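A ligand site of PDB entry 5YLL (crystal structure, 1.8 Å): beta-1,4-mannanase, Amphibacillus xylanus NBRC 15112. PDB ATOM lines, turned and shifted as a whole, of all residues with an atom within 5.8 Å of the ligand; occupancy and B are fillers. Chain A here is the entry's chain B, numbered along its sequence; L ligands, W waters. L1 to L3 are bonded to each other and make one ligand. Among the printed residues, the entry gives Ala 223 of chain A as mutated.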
ATOM      1  N   TRP A  11      16.614 -29.683  -7.436  1.00  0.00           N
ATOM      2  CA  TRP A  11      17.542 -28.747  -6.795  1.00  0.00           C
ATOM      3  C   TRP A  11      17.893 -29.180  -5.385  1.00  0.00           C
ATOM      4  O   TRP A  11      19.008 -28.900  -4.913  1.00  0.00           O
ATOM      5  CB  TRP A  11      16.933 -27.348  -6.767  1.00  0.00           C
ATOM      6  CG  TRP A  11      17.867 -26.246  -6.312  1.00  0.00           C
ATOM      7  CD1 TRP A  11      17.665 -25.413  -5.258  1.00  0.00           C
ATOM      8  CD2 TRP A  11      19.098 -25.845  -6.927  1.00  0.00           C
ATOM      9  NE1 TRP A  11      18.698 -24.500  -5.170  1.00  0.00           N
ATOM     10  CE2 TRP A  11      19.588 -24.751  -6.189  1.00  0.00           C
ATOM     11  CE3 TRP A  11      19.821 -26.290  -8.039  1.00  0.00           C
ATOM     12  CZ2 TRP A  11      20.775 -24.094  -6.508  1.00  0.00           C
ATOM     13  CZ3 TRP A  11      21.012 -25.647  -8.358  1.00  0.00           C
ATOM     14  CH2 TRP A  11      21.484 -24.558  -7.590  1.00  0.00           C
ATOM     15  N   LYS A  85      20.932 -28.646 -16.338  1.00  0.00           N
ATOM     16  CA  LYS A  85      21.452 -27.362 -15.863  1.00  0.00           C
ATOM     17  C   LYS A  85      22.419 -27.603 -14.711  1.00  0.00           C
ATOM     18  O   LYS A  85      22.045 -27.517 -13.539  1.00  0.00           O
ATOM     19  CB  LYS A  85      20.314 -26.437 -15.444  1.00  0.00           C
ATOM     20  CG  LYS A  85      20.744 -25.012 -15.026  1.00  0.00           C
ATOM     21  CD  LYS A  85      19.508 -24.074 -14.990  1.00  0.00           C
ATOM     22  CE  LYS A  85      19.368 -23.396 -13.659  1.00  0.00           C
ATOM     23  NZ  LYS A  85      18.334 -22.315 -13.716  1.00  0.00           N
ATOM     24  N   ASN A  89      27.550 -24.045  -6.434  1.00  0.00           N
ATOM     25  CA  ASN A  89      27.331 -23.265  -5.228  1.00  0.00           C
ATOM     26  C   ASN A  89      28.616 -23.219  -4.422  1.00  0.00           C
ATOM     27  O   ASN A  89      29.542 -23.989  -4.643  1.00  0.00           O
ATOM     28  CB  ASN A  89      26.193 -23.862  -4.380  1.00  0.00           C
ATOM     29  CG  ASN A  89      24.826 -23.685  -5.035  1.00  0.00           C
ATOM     30  OD1 ASN A  89      24.602 -22.738  -5.791  1.00  0.00           O
ATOM     31  ND2 ASN A  89      23.907 -24.599  -4.747  1.00  0.00           N
ATOM     32  N   TRP A  95      26.570 -16.444  -2.883  1.00  0.00           N
ATOM     33  CA  TRP A  95      25.914 -16.613  -4.183  1.00  0.00           C
ATOM     34  C   TRP A  95      26.948 -16.668  -5.307  1.00  0.00           C
ATOM     35  O   TRP A  95      27.880 -15.868  -5.354  1.00  0.00           O
ATOM     36  CB  TRP A  95      24.944 -15.448  -4.391  1.00  0.00           C
ATOM     37  CG  TRP A  95      24.127 -15.452  -5.645  1.00  0.00           C
ATOM     38  CD1 TRP A  95      23.712 -16.530  -6.383  1.00  0.00           C
ATOM     39  CD2 TRP A  95      23.574 -14.302  -6.265  1.00  0.00           C
ATOM     40  NE1 TRP A  95      22.949 -16.093  -7.448  1.00  0.00           N
ATOM     41  CE2 TRP A  95      22.853 -14.731  -7.403  1.00  0.00           C
ATOM     42  CE3 TRP A  95      23.623 -12.929  -5.989  1.00  0.00           C
ATOM     43  CZ2 TRP A  95      22.186 -13.845  -8.253  1.00  0.00           C
ATOM     44  CZ3 TRP A  95      22.963 -12.048  -6.842  1.00  0.00           C
ATOM     45  CH2 TRP A  95      22.248 -12.506  -7.948  1.00  0.00           C
ATOM     46  N   ARG A  96      26.764 -17.630  -6.213  1.00  0.00           N
ATOM     47  CA  ARG A  96      27.719 -17.856  -7.304  1.00  0.00           C
ATOM     48  C   ARG A  96      27.896 -16.646  -8.211  1.00  0.00           C
ATOM     49  O   ARG A  96      28.914 -16.566  -8.913  1.00  0.00           O
ATOM     50  CB  ARG A  96      27.265 -19.069  -8.137  1.00  0.00           C
ATOM     51  CG  ARG A  96      26.051 -18.791  -9.036  1.00  0.00           C
ATOM     52  CD  ARG A  96      25.461 -20.086  -9.644  1.00  0.00           C
ATOM     53  NE  ARG A  96      24.727 -20.859  -8.650  1.00  0.00           N
ATOM     54  CZ  ARG A  96      23.473 -20.604  -8.271  1.00  0.00           C
ATOM     55  NH1 ARG A  96      22.800 -19.620  -8.842  1.00  0.00           N
ATOM     56  NH2 ARG A  96      22.920 -21.334  -7.312  1.00  0.00           N
ATOM     57  N   CYS A 142      24.826 -20.368 -14.789  1.00  0.00           N
ATOM     58  CA  CYS A 142      23.611 -19.808 -14.185  1.00  0.00           C
ATOM     59  C   CYS A 142      24.020 -18.635 -13.298  1.00  0.00           C
ATOM     60  O   CYS A 142      24.724 -18.836 -12.311  1.00  0.00           O
ATOM     61  CB  CYS A 142      22.878 -20.892 -13.400  1.00  0.00           C
ATOM     62  SG  CYS A 142      21.519 -20.327 -12.378  1.00  0.00           S
ATOM     63  N   GLU A 143      23.586 -17.430 -13.668  1.00  0.00           N
ATOM     64  CA  GLU A 143      23.692 -16.253 -12.785  1.00  0.00           C
ATOM     65  C   GLU A 143      25.151 -15.958 -12.404  1.00  0.00           C
ATOM     66  O   GLU A 143      25.432 -15.503 -11.300  1.00  0.00           O
ATOM     67  CB  GLU A 143      22.830 -16.418 -11.514  1.00  0.00           C
ATOM     68  CG  GLU A 143      21.314 -16.426 -11.759  1.00  0.00           C
ATOM     69  CD  GLU A 143      20.486 -17.015 -10.607  1.00  0.00           C
ATOM     70  OE1 GLU A 143      19.245 -17.088 -10.745  1.00  0.00           O
ATOM     71  OE2 GLU A 143      21.038 -17.383  -9.555  1.00  0.00           O
ATOM     72  N   ASN A 172      22.272 -18.957 -18.703  1.00  0.00           N
ATOM     73  CA  ASN A 172      21.170 -18.392 -17.908  1.00  0.00           C
ATOM     74  C   ASN A 172      21.728 -17.203 -17.161  1.00  0.00           C
ATOM     75  O   ASN A 172      22.490 -17.360 -16.199  1.00  0.00           O
ATOM     76  CB  ASN A 172      20.620 -19.497 -17.003  1.00  0.00           C
ATOM     77  CG  ASN A 172      19.683 -19.013 -15.892  1.00  0.00           C
ATOM     78  OD1 ASN A 172      19.424 -19.763 -14.956  1.00  0.00           O
ATOM     79  ND2 ASN A 172      19.118 -17.817 -16.022  1.00  0.00           N
ATOM     80  N   SER A 193      17.011 -15.514 -15.617  1.00  0.00           N
ATOM     81  CA  SER A 193      16.201 -15.716 -14.409  1.00  0.00           C
ATOM     82  C   SER A 193      15.224 -14.563 -14.277  1.00  0.00           C
ATOM     83  O   SER A 193      15.568 -13.518 -13.703  1.00  0.00           O
ATOM     84  CB  SER A 193      17.100 -15.787 -13.174  1.00  0.00           C
ATOM     85  OG  SER A 193      17.940 -16.917 -13.174  1.00  0.00           O
ATOM     86  N   TYR A 195      13.054 -13.091 -12.472  1.00  0.00           N
ATOM     87  CA  TYR A 195      12.482 -12.800 -11.154  1.00  0.00           C
ATOM     88  C   TYR A 195      12.139 -11.315 -11.047  1.00  0.00           C
ATOM     89  O   TYR A 195      12.747 -10.557 -10.294  1.00  0.00           O
ATOM     90  CB  TYR A 195      13.462 -13.210 -10.063  1.00  0.00           C
ATOM     91  CG  TYR A 195      13.666 -14.693  -9.906  1.00  0.00           C
ATOM     92  CD1 TYR A 195      12.606 -15.529  -9.629  1.00  0.00           C
ATOM     93  CD2 TYR A 195      14.947 -15.243  -9.951  1.00  0.00           C
ATOM     94  CE1 TYR A 195      12.782 -16.881  -9.446  1.00  0.00           C
ATOM     95  CE2 TYR A 195      15.139 -16.591  -9.765  1.00  0.00           C
ATOM     96  CZ  TYR A 195      14.056 -17.410  -9.512  1.00  0.00           C
ATOM     97  OH  TYR A 195      14.236 -18.762  -9.321  1.00  0.00           O
ATOM     98  N   ALA A 223      14.565 -19.735 -15.467  1.00  0.00           N
ATOM     99  CA  ALA A 223      14.082 -19.760 -14.081  1.00  0.00           C
ATOM    100  C   ALA A 223      13.119 -18.592 -13.869  1.00  0.00           C
ATOM    101  O   ALA A 223      13.345 -17.494 -14.377  1.00  0.00           O
ATOM    102  CB  ALA A 223      15.222 -19.683 -13.042  1.00  0.00           C
ATOM    103  N   PRO A 236      10.792 -11.624  -5.960  1.00  0.00           N
ATOM    104  CA  PRO A 236      10.561 -13.076  -5.970  1.00  0.00           C
ATOM    105  C   PRO A 236      11.833 -13.918  -6.016  1.00  0.00           C
ATOM    106  O   PRO A 236      11.748 -15.140  -5.852  1.00  0.00           O
ATOM    107  CB  PRO A 236       9.718 -13.274  -7.245  1.00  0.00           C
ATOM    108  CG  PRO A 236      10.072 -12.098  -8.127  1.00  0.00           C
ATOM    109  CD  PRO A 236      10.379 -10.950  -7.196  1.00  0.00           C
ATOM    110  N   ASN A 237      12.997 -13.307  -6.214  1.00  0.00           N
ATOM    111  CA  ASN A 237      14.275 -14.027  -6.195  1.00  0.00           C
ATOM    112  C   ASN A 237      14.784 -14.308  -4.773  1.00  0.00           C
ATOM    113  O   ASN A 237      15.703 -15.128  -4.619  1.00  0.00           O
ATOM    114  CB  ASN A 237      15.335 -13.219  -6.926  1.00  0.00           C
ATOM    115  CG  ASN A 237      15.532 -11.847  -6.288  1.00  0.00           C
ATOM    116  OD1 ASN A 237      14.631 -11.006  -6.299  1.00  0.00           O
ATOM    117  ND2 ASN A 237      16.718 -11.627  -5.723  1.00  0.00           N
ATOM    118  N   LYS A 238      14.257 -13.635  -3.758  1.00  0.00           N
ATOM    119  CA  LYS A 238      14.822 -13.733  -2.414  1.00  0.00           C
ATOM    120  C   LYS A 238      14.209 -14.947  -1.715  1.00  0.00           C
ATOM    121  O   LYS A 238      13.097 -14.869  -1.179  1.00  0.00           O
ATOM    122  CB  LYS A 238      14.576 -12.437  -1.641  1.00  0.00           C
ATOM    123  CG  LYS A 238      15.326 -11.254  -2.222  1.00  0.00           C
ATOM    124  CD  LYS A 238      15.841 -10.340  -1.125  1.00  0.00           C
ATOM    125  CE  LYS A 238      17.220  -9.778  -1.475  1.00  0.00           C
ATOM    126  NZ  LYS A 238      17.996  -9.390  -0.249  1.00  0.00           N
ATOM    127  N   TRP A 239      14.919 -16.063  -1.716  1.00  0.00           N
ATOM    128  CA  TRP A 239      14.352 -17.250  -1.081  1.00  0.00           C
ATOM    129  C   TRP A 239      14.320 -17.149   0.435  1.00  0.00           C
ATOM    130  O   TRP A 239      13.660 -17.973   1.076  1.00  0.00           O
ATOM    131  CB  TRP A 239      15.138 -18.503  -1.474  1.00  0.00           C
ATOM    132  CG  TRP A 239      16.486 -18.477  -0.932  1.00  0.00           C
ATOM    133  CD1 TRP A 239      16.892 -18.906   0.314  1.00  0.00           C
ATOM    134  CD2 TRP A 239      17.648 -17.975  -1.579  1.00  0.00           C
ATOM    135  NE1 TRP A 239      18.233 -18.709   0.458  1.00  0.00           N
ATOM    136  CE2 TRP A 239      18.723 -18.132  -0.694  1.00  0.00           C
ATOM    137  CE3 TRP A 239      17.879 -17.409  -2.828  1.00  0.00           C
ATOM    138  CZ2 TRP A 239      20.009 -17.758  -1.016  1.00  0.00           C
ATOM    139  CZ3 TRP A 239      19.157 -17.030  -3.146  1.00  0.00           C
ATOM    140  CH2 TRP A 239      20.202 -17.201  -2.248  1.00  0.00           C
ATOM    141  N   TRP A 273      10.502 -22.282 -11.063  1.00  0.00           N
ATOM    142  CA  TRP A 273      11.320 -22.600  -9.898  1.00  0.00           C
ATOM    143  C   TRP A 273      10.405 -22.717  -8.684  1.00  0.00           C
ATOM    144  O   TRP A 273       9.736 -21.734  -8.334  1.00  0.00           O
ATOM    145  CB  TRP A 273      12.358 -21.503  -9.661  1.00  0.00           C
ATOM    146  CG  TRP A 273      13.406 -21.950  -8.726  1.00  0.00           C
ATOM    147  CD1 TRP A 273      13.343 -21.960  -7.364  1.00  0.00           C
ATOM    148  CD2 TRP A 273      14.670 -22.523  -9.078  1.00  0.00           C
ATOM    149  NE1 TRP A 273      14.492 -22.493  -6.845  1.00  0.00           N
ATOM    150  CE2 TRP A 273      15.326 -22.844  -7.867  1.00  0.00           C
ATOM    151  CE3 TRP A 273      15.312 -22.773 -10.286  1.00  0.00           C
ATOM    152  CZ2 TRP A 273      16.599 -23.405  -7.844  1.00  0.00           C
ATOM    153  CZ3 TRP A 273      16.576 -23.351 -10.258  1.00  0.00           C
ATOM    154  CH2 TRP A 273      17.208 -23.655  -9.039  1.00  0.00           C
ATOM    155  N   ASP A 274      10.355 -23.882  -8.028  1.00  0.00           N
ATOM    156  CA  ASP A 274      11.001 -25.138  -8.417  1.00  0.00           C
ATOM    157  C   ASP A 274      10.173 -26.259  -7.818  1.00  0.00           C
ATOM    158  O   ASP A 274       9.309 -26.004  -6.973  1.00  0.00           O
ATOM    159  CB  ASP A 274      12.471 -25.221  -7.930  1.00  0.00           C
ATOM    160  CG  ASP A 274      12.602 -25.474  -6.417  1.00  0.00           C
ATOM    161  OD1 ASP A 274      11.917 -24.808  -5.606  1.00  0.00           O
ATOM    162  OD2 ASP A 274      13.430 -26.330  -6.038  1.00  0.00           O
ATOM    163  N   TYR A 291       9.082 -22.023  -2.658  1.00  0.00           N
ATOM    164  CA  TYR A 291       8.741 -21.834  -4.069  1.00  0.00           C
ATOM    165  C   TYR A 291       7.774 -22.869  -4.601  1.00  0.00           C
ATOM    166  O   TYR A 291       7.115 -22.621  -5.621  1.00  0.00           O
ATOM    167  CB  TYR A 291      10.012 -21.895  -4.922  1.00  0.00           C
ATOM    168  CG  TYR A 291      10.842 -20.643  -4.879  1.00  0.00           C
ATOM    169  CD1 TYR A 291      10.610 -19.592  -5.779  1.00  0.00           C
ATOM    170  CD2 TYR A 291      11.872 -20.499  -3.950  1.00  0.00           C
ATOM    171  CE1 TYR A 291      11.389 -18.431  -5.741  1.00  0.00           C
ATOM    172  CE2 TYR A 291      12.638 -19.341  -3.907  1.00  0.00           C
ATOM    173  CZ  TYR A 291      12.400 -18.321  -4.802  1.00  0.00           C
ATOM    174  OH  TYR A 291      13.157 -17.171  -4.765  1.00  0.00           O
HETATM  175  C1  LIG L   1      17.693 -19.787  -8.847  1.00  0.00           C
HETATM  176  C2  LIG L   1      19.069 -19.847  -8.181  1.00  0.00           C
HETATM  177  C3  LIG L   1      18.961 -20.561  -6.877  1.00  0.00           C
HETATM  178  C4  LIG L   1      17.893 -19.992  -5.965  1.00  0.00           C
HETATM  179  C5  LIG L   1      16.562 -19.854  -6.720  1.00  0.00           C
HETATM  180  C6  LIG L   1      15.475 -19.153  -5.961  1.00  0.00           C
HETATM  181  O1  LIG L   1      17.700 -19.129 -10.052  1.00  0.00           O
HETATM  182  O2  LIG L   1      19.541 -18.509  -7.895  1.00  0.00           O
HETATM  183  O3  LIG L   1      20.252 -20.538  -6.213  1.00  0.00           O
HETATM  184  O4  LIG L   1      17.489 -21.017  -4.953  1.00  0.00           O
HETATM  185  O5  LIG L   1      16.768 -19.063  -7.940  1.00  0.00           O
HETATM  186  O6  LIG L   1      15.933 -17.904  -5.523  1.00  0.00           O
HETATM  187  C1  LG2 L   2      18.162 -20.999  -3.770  1.00  0.00           C
HETATM  188  C2  LG2 L   2      17.372 -21.707  -2.669  1.00  0.00           C
HETATM  189  C3  LG2 L   2      18.186 -21.747  -1.411  1.00  0.00           C
HETATM  190  C4  LG2 L   2      19.559 -22.337  -1.613  1.00  0.00           C
HETATM  191  C5  LG2 L   2      20.298 -21.666  -2.777  1.00  0.00           C
HETATM  192  C6  LG2 L   2      21.563 -22.391  -3.120  1.00  0.00           C
HETATM  193  O1  LG2 L   2      17.056 -23.048  -3.107  1.00  0.00           O
HETATM  194  O2  LG2 L   2      17.481 -22.514  -0.386  1.00  0.00           O
HETATM  195  O3  LG2 L   2      20.426 -22.445  -0.525  1.00  0.00           O
HETATM  196  O4  LG2 L   2      19.457 -21.700  -3.975  1.00  0.00           O
HETATM  197  O5  LG2 L   2      22.200 -21.740  -4.186  1.00  0.00           O
HETATM  198  C1  LG3 L   3      20.824 -23.656  -0.042  1.00  0.00           C
HETATM  199  C2  LG3 L   3      21.872 -23.477   1.040  1.00  0.00           C
HETATM  200  C3  LG3 L   3      22.272 -24.785   1.636  1.00  0.00           C
HETATM  201  C4  LG3 L   3      21.097 -25.610   2.091  1.00  0.00           C
HETATM  202  C5  LG3 L   3      19.960 -25.687   1.061  1.00  0.00           C
HETATM  203  C6  LG3 L   3      18.750 -26.273   1.733  1.00  0.00           C
HETATM  204  O1  LG3 L   3      21.344 -22.630   2.077  1.00  0.00           O
HETATM  205  O2  LG3 L   3      23.167 -24.555   2.757  1.00  0.00           O
HETATM  206  O3  LG3 L   3      21.132 -27.151   2.647  1.00  0.00           O
HETATM  207  O4  LG3 L   3      19.623 -24.359   0.492  1.00  0.00           O
HETATM  208  O5  LG3 L   3      17.600 -26.087   0.965  1.00  0.00           O
HETATM  209  O   HOH W   1      18.613 -20.406 -12.082  1.00  0.00           O
HETATM  210  O   HOH W   2      14.547 -23.180  -3.982  1.00  0.00           O
HETATM  211  O   HOH W   3      17.803 -16.325  -7.106  1.00  0.00           O
HETATM  212  O   HOH W   4      22.657 -19.183  -4.022  1.00  0.00           O
HETATM  213  O   HOH W   5      21.010 -17.756  -5.559  1.00  0.00           O
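The side-chain carboxylate of Glu 143 lies within hydrogen-bond range of an oxygen (O2) of LIG L1 (2.5 Å). OH of Tyr 195 lies within hydrogen-bond range of O5 of LIG L1, 2.9 Å away. An oxygen (O6) of LIG L1 sits at hydrogen-bond distance from the backbone carbonyl oxygen (O) of Asn 237. OH of Tyr 291 sits at hydrogen-bond distance from O6 of LIG L1 (3.0 Å). NH2 of Arg 96 is in hydrogen-bond range of O3 of LIG L1 (3.0 Å). O1 of LG2 L2 lies within hydrogen-bond range of NE1 of Trp 11. The side-chain amide oxygen of Asn 89 sits at hydrogen-bond distance from an oxygen (O5) of LG2 L2 (3.1 Å).
Water W1 lies within hydrogen-bond range of NZ of Lys 85 (2.5 Å), O1 of LIG L1 (2.6 Å), SG of Cys 142 (2.9 Å) and OD1 of Asn 172 (3.1 Å). Water W2 lies within hydrogen-bond range of an oxygen (O1) of LG2 L2, the indole nitrogen of Trp 273 and the side-chain carboxylate of Asp 274. Water W5 lies within hydrogen-bond range of O2 of LIG L1 (2.9 Å) and NE1 of Trp 95 (3.2 Å). Water W3 lies within hydrogen-bond range of an oxygen (O2) of LIG L1 (2.9 Å) and the backbone carbonyl oxygen of Asn 237 (3.5 Å).
OE2 of Glu 143 lies within salt-bridge range of NH1 of Arg 96, 2.9 Å away. OE1 of Glu 143 is in hydrogen-bond range of OG of Ser 193 (2.8 Å). The indole nitrogen (NE1) of Trp 95 is in hydrogen-bond range of the side-chain carboxylate (OE2) of Glu 143 (3.1 Å). The backbone carbonyl oxygen (O) of Asn 172 lies within hydrogen-bond range of the backbone NH (N) of Glu 143, 2.8 Å away. The side-chain hydroxyl (OH) of Tyr 291 sits at hydrogen-bond distance from the backbone carbonyl oxygen (O) of Asn 237, 3.3 Å away. O of Pro 236 lies within hydrogen-bond range of OH of Tyr 291, at 2.7 Å. NH2 of Arg 96 lies within hydrogen-bond range of OD1 of Asn 89 (2.7 Å). N of Ser 193 lies close to ND2 of Asn 172 (3.1 Å).
Ser 193 touches the ligand. CB of Ala 223 touches O1 of LIG L1 (3.9 Å). CE3 of Trp 239 touches O6 of LIG L1, 3.4 Å away. NE1 of Trp 273 touches C5 of LIG L1, 3.4 Å away. Hydrophobic or aromatic side chains within 4 Å of the ligand: Trp 11, Tyr 195, Ala 223, Trp 239, Trp 273 and Tyr 291. Of the 18 residues printed, 11 come within 4 Å of the ligand.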
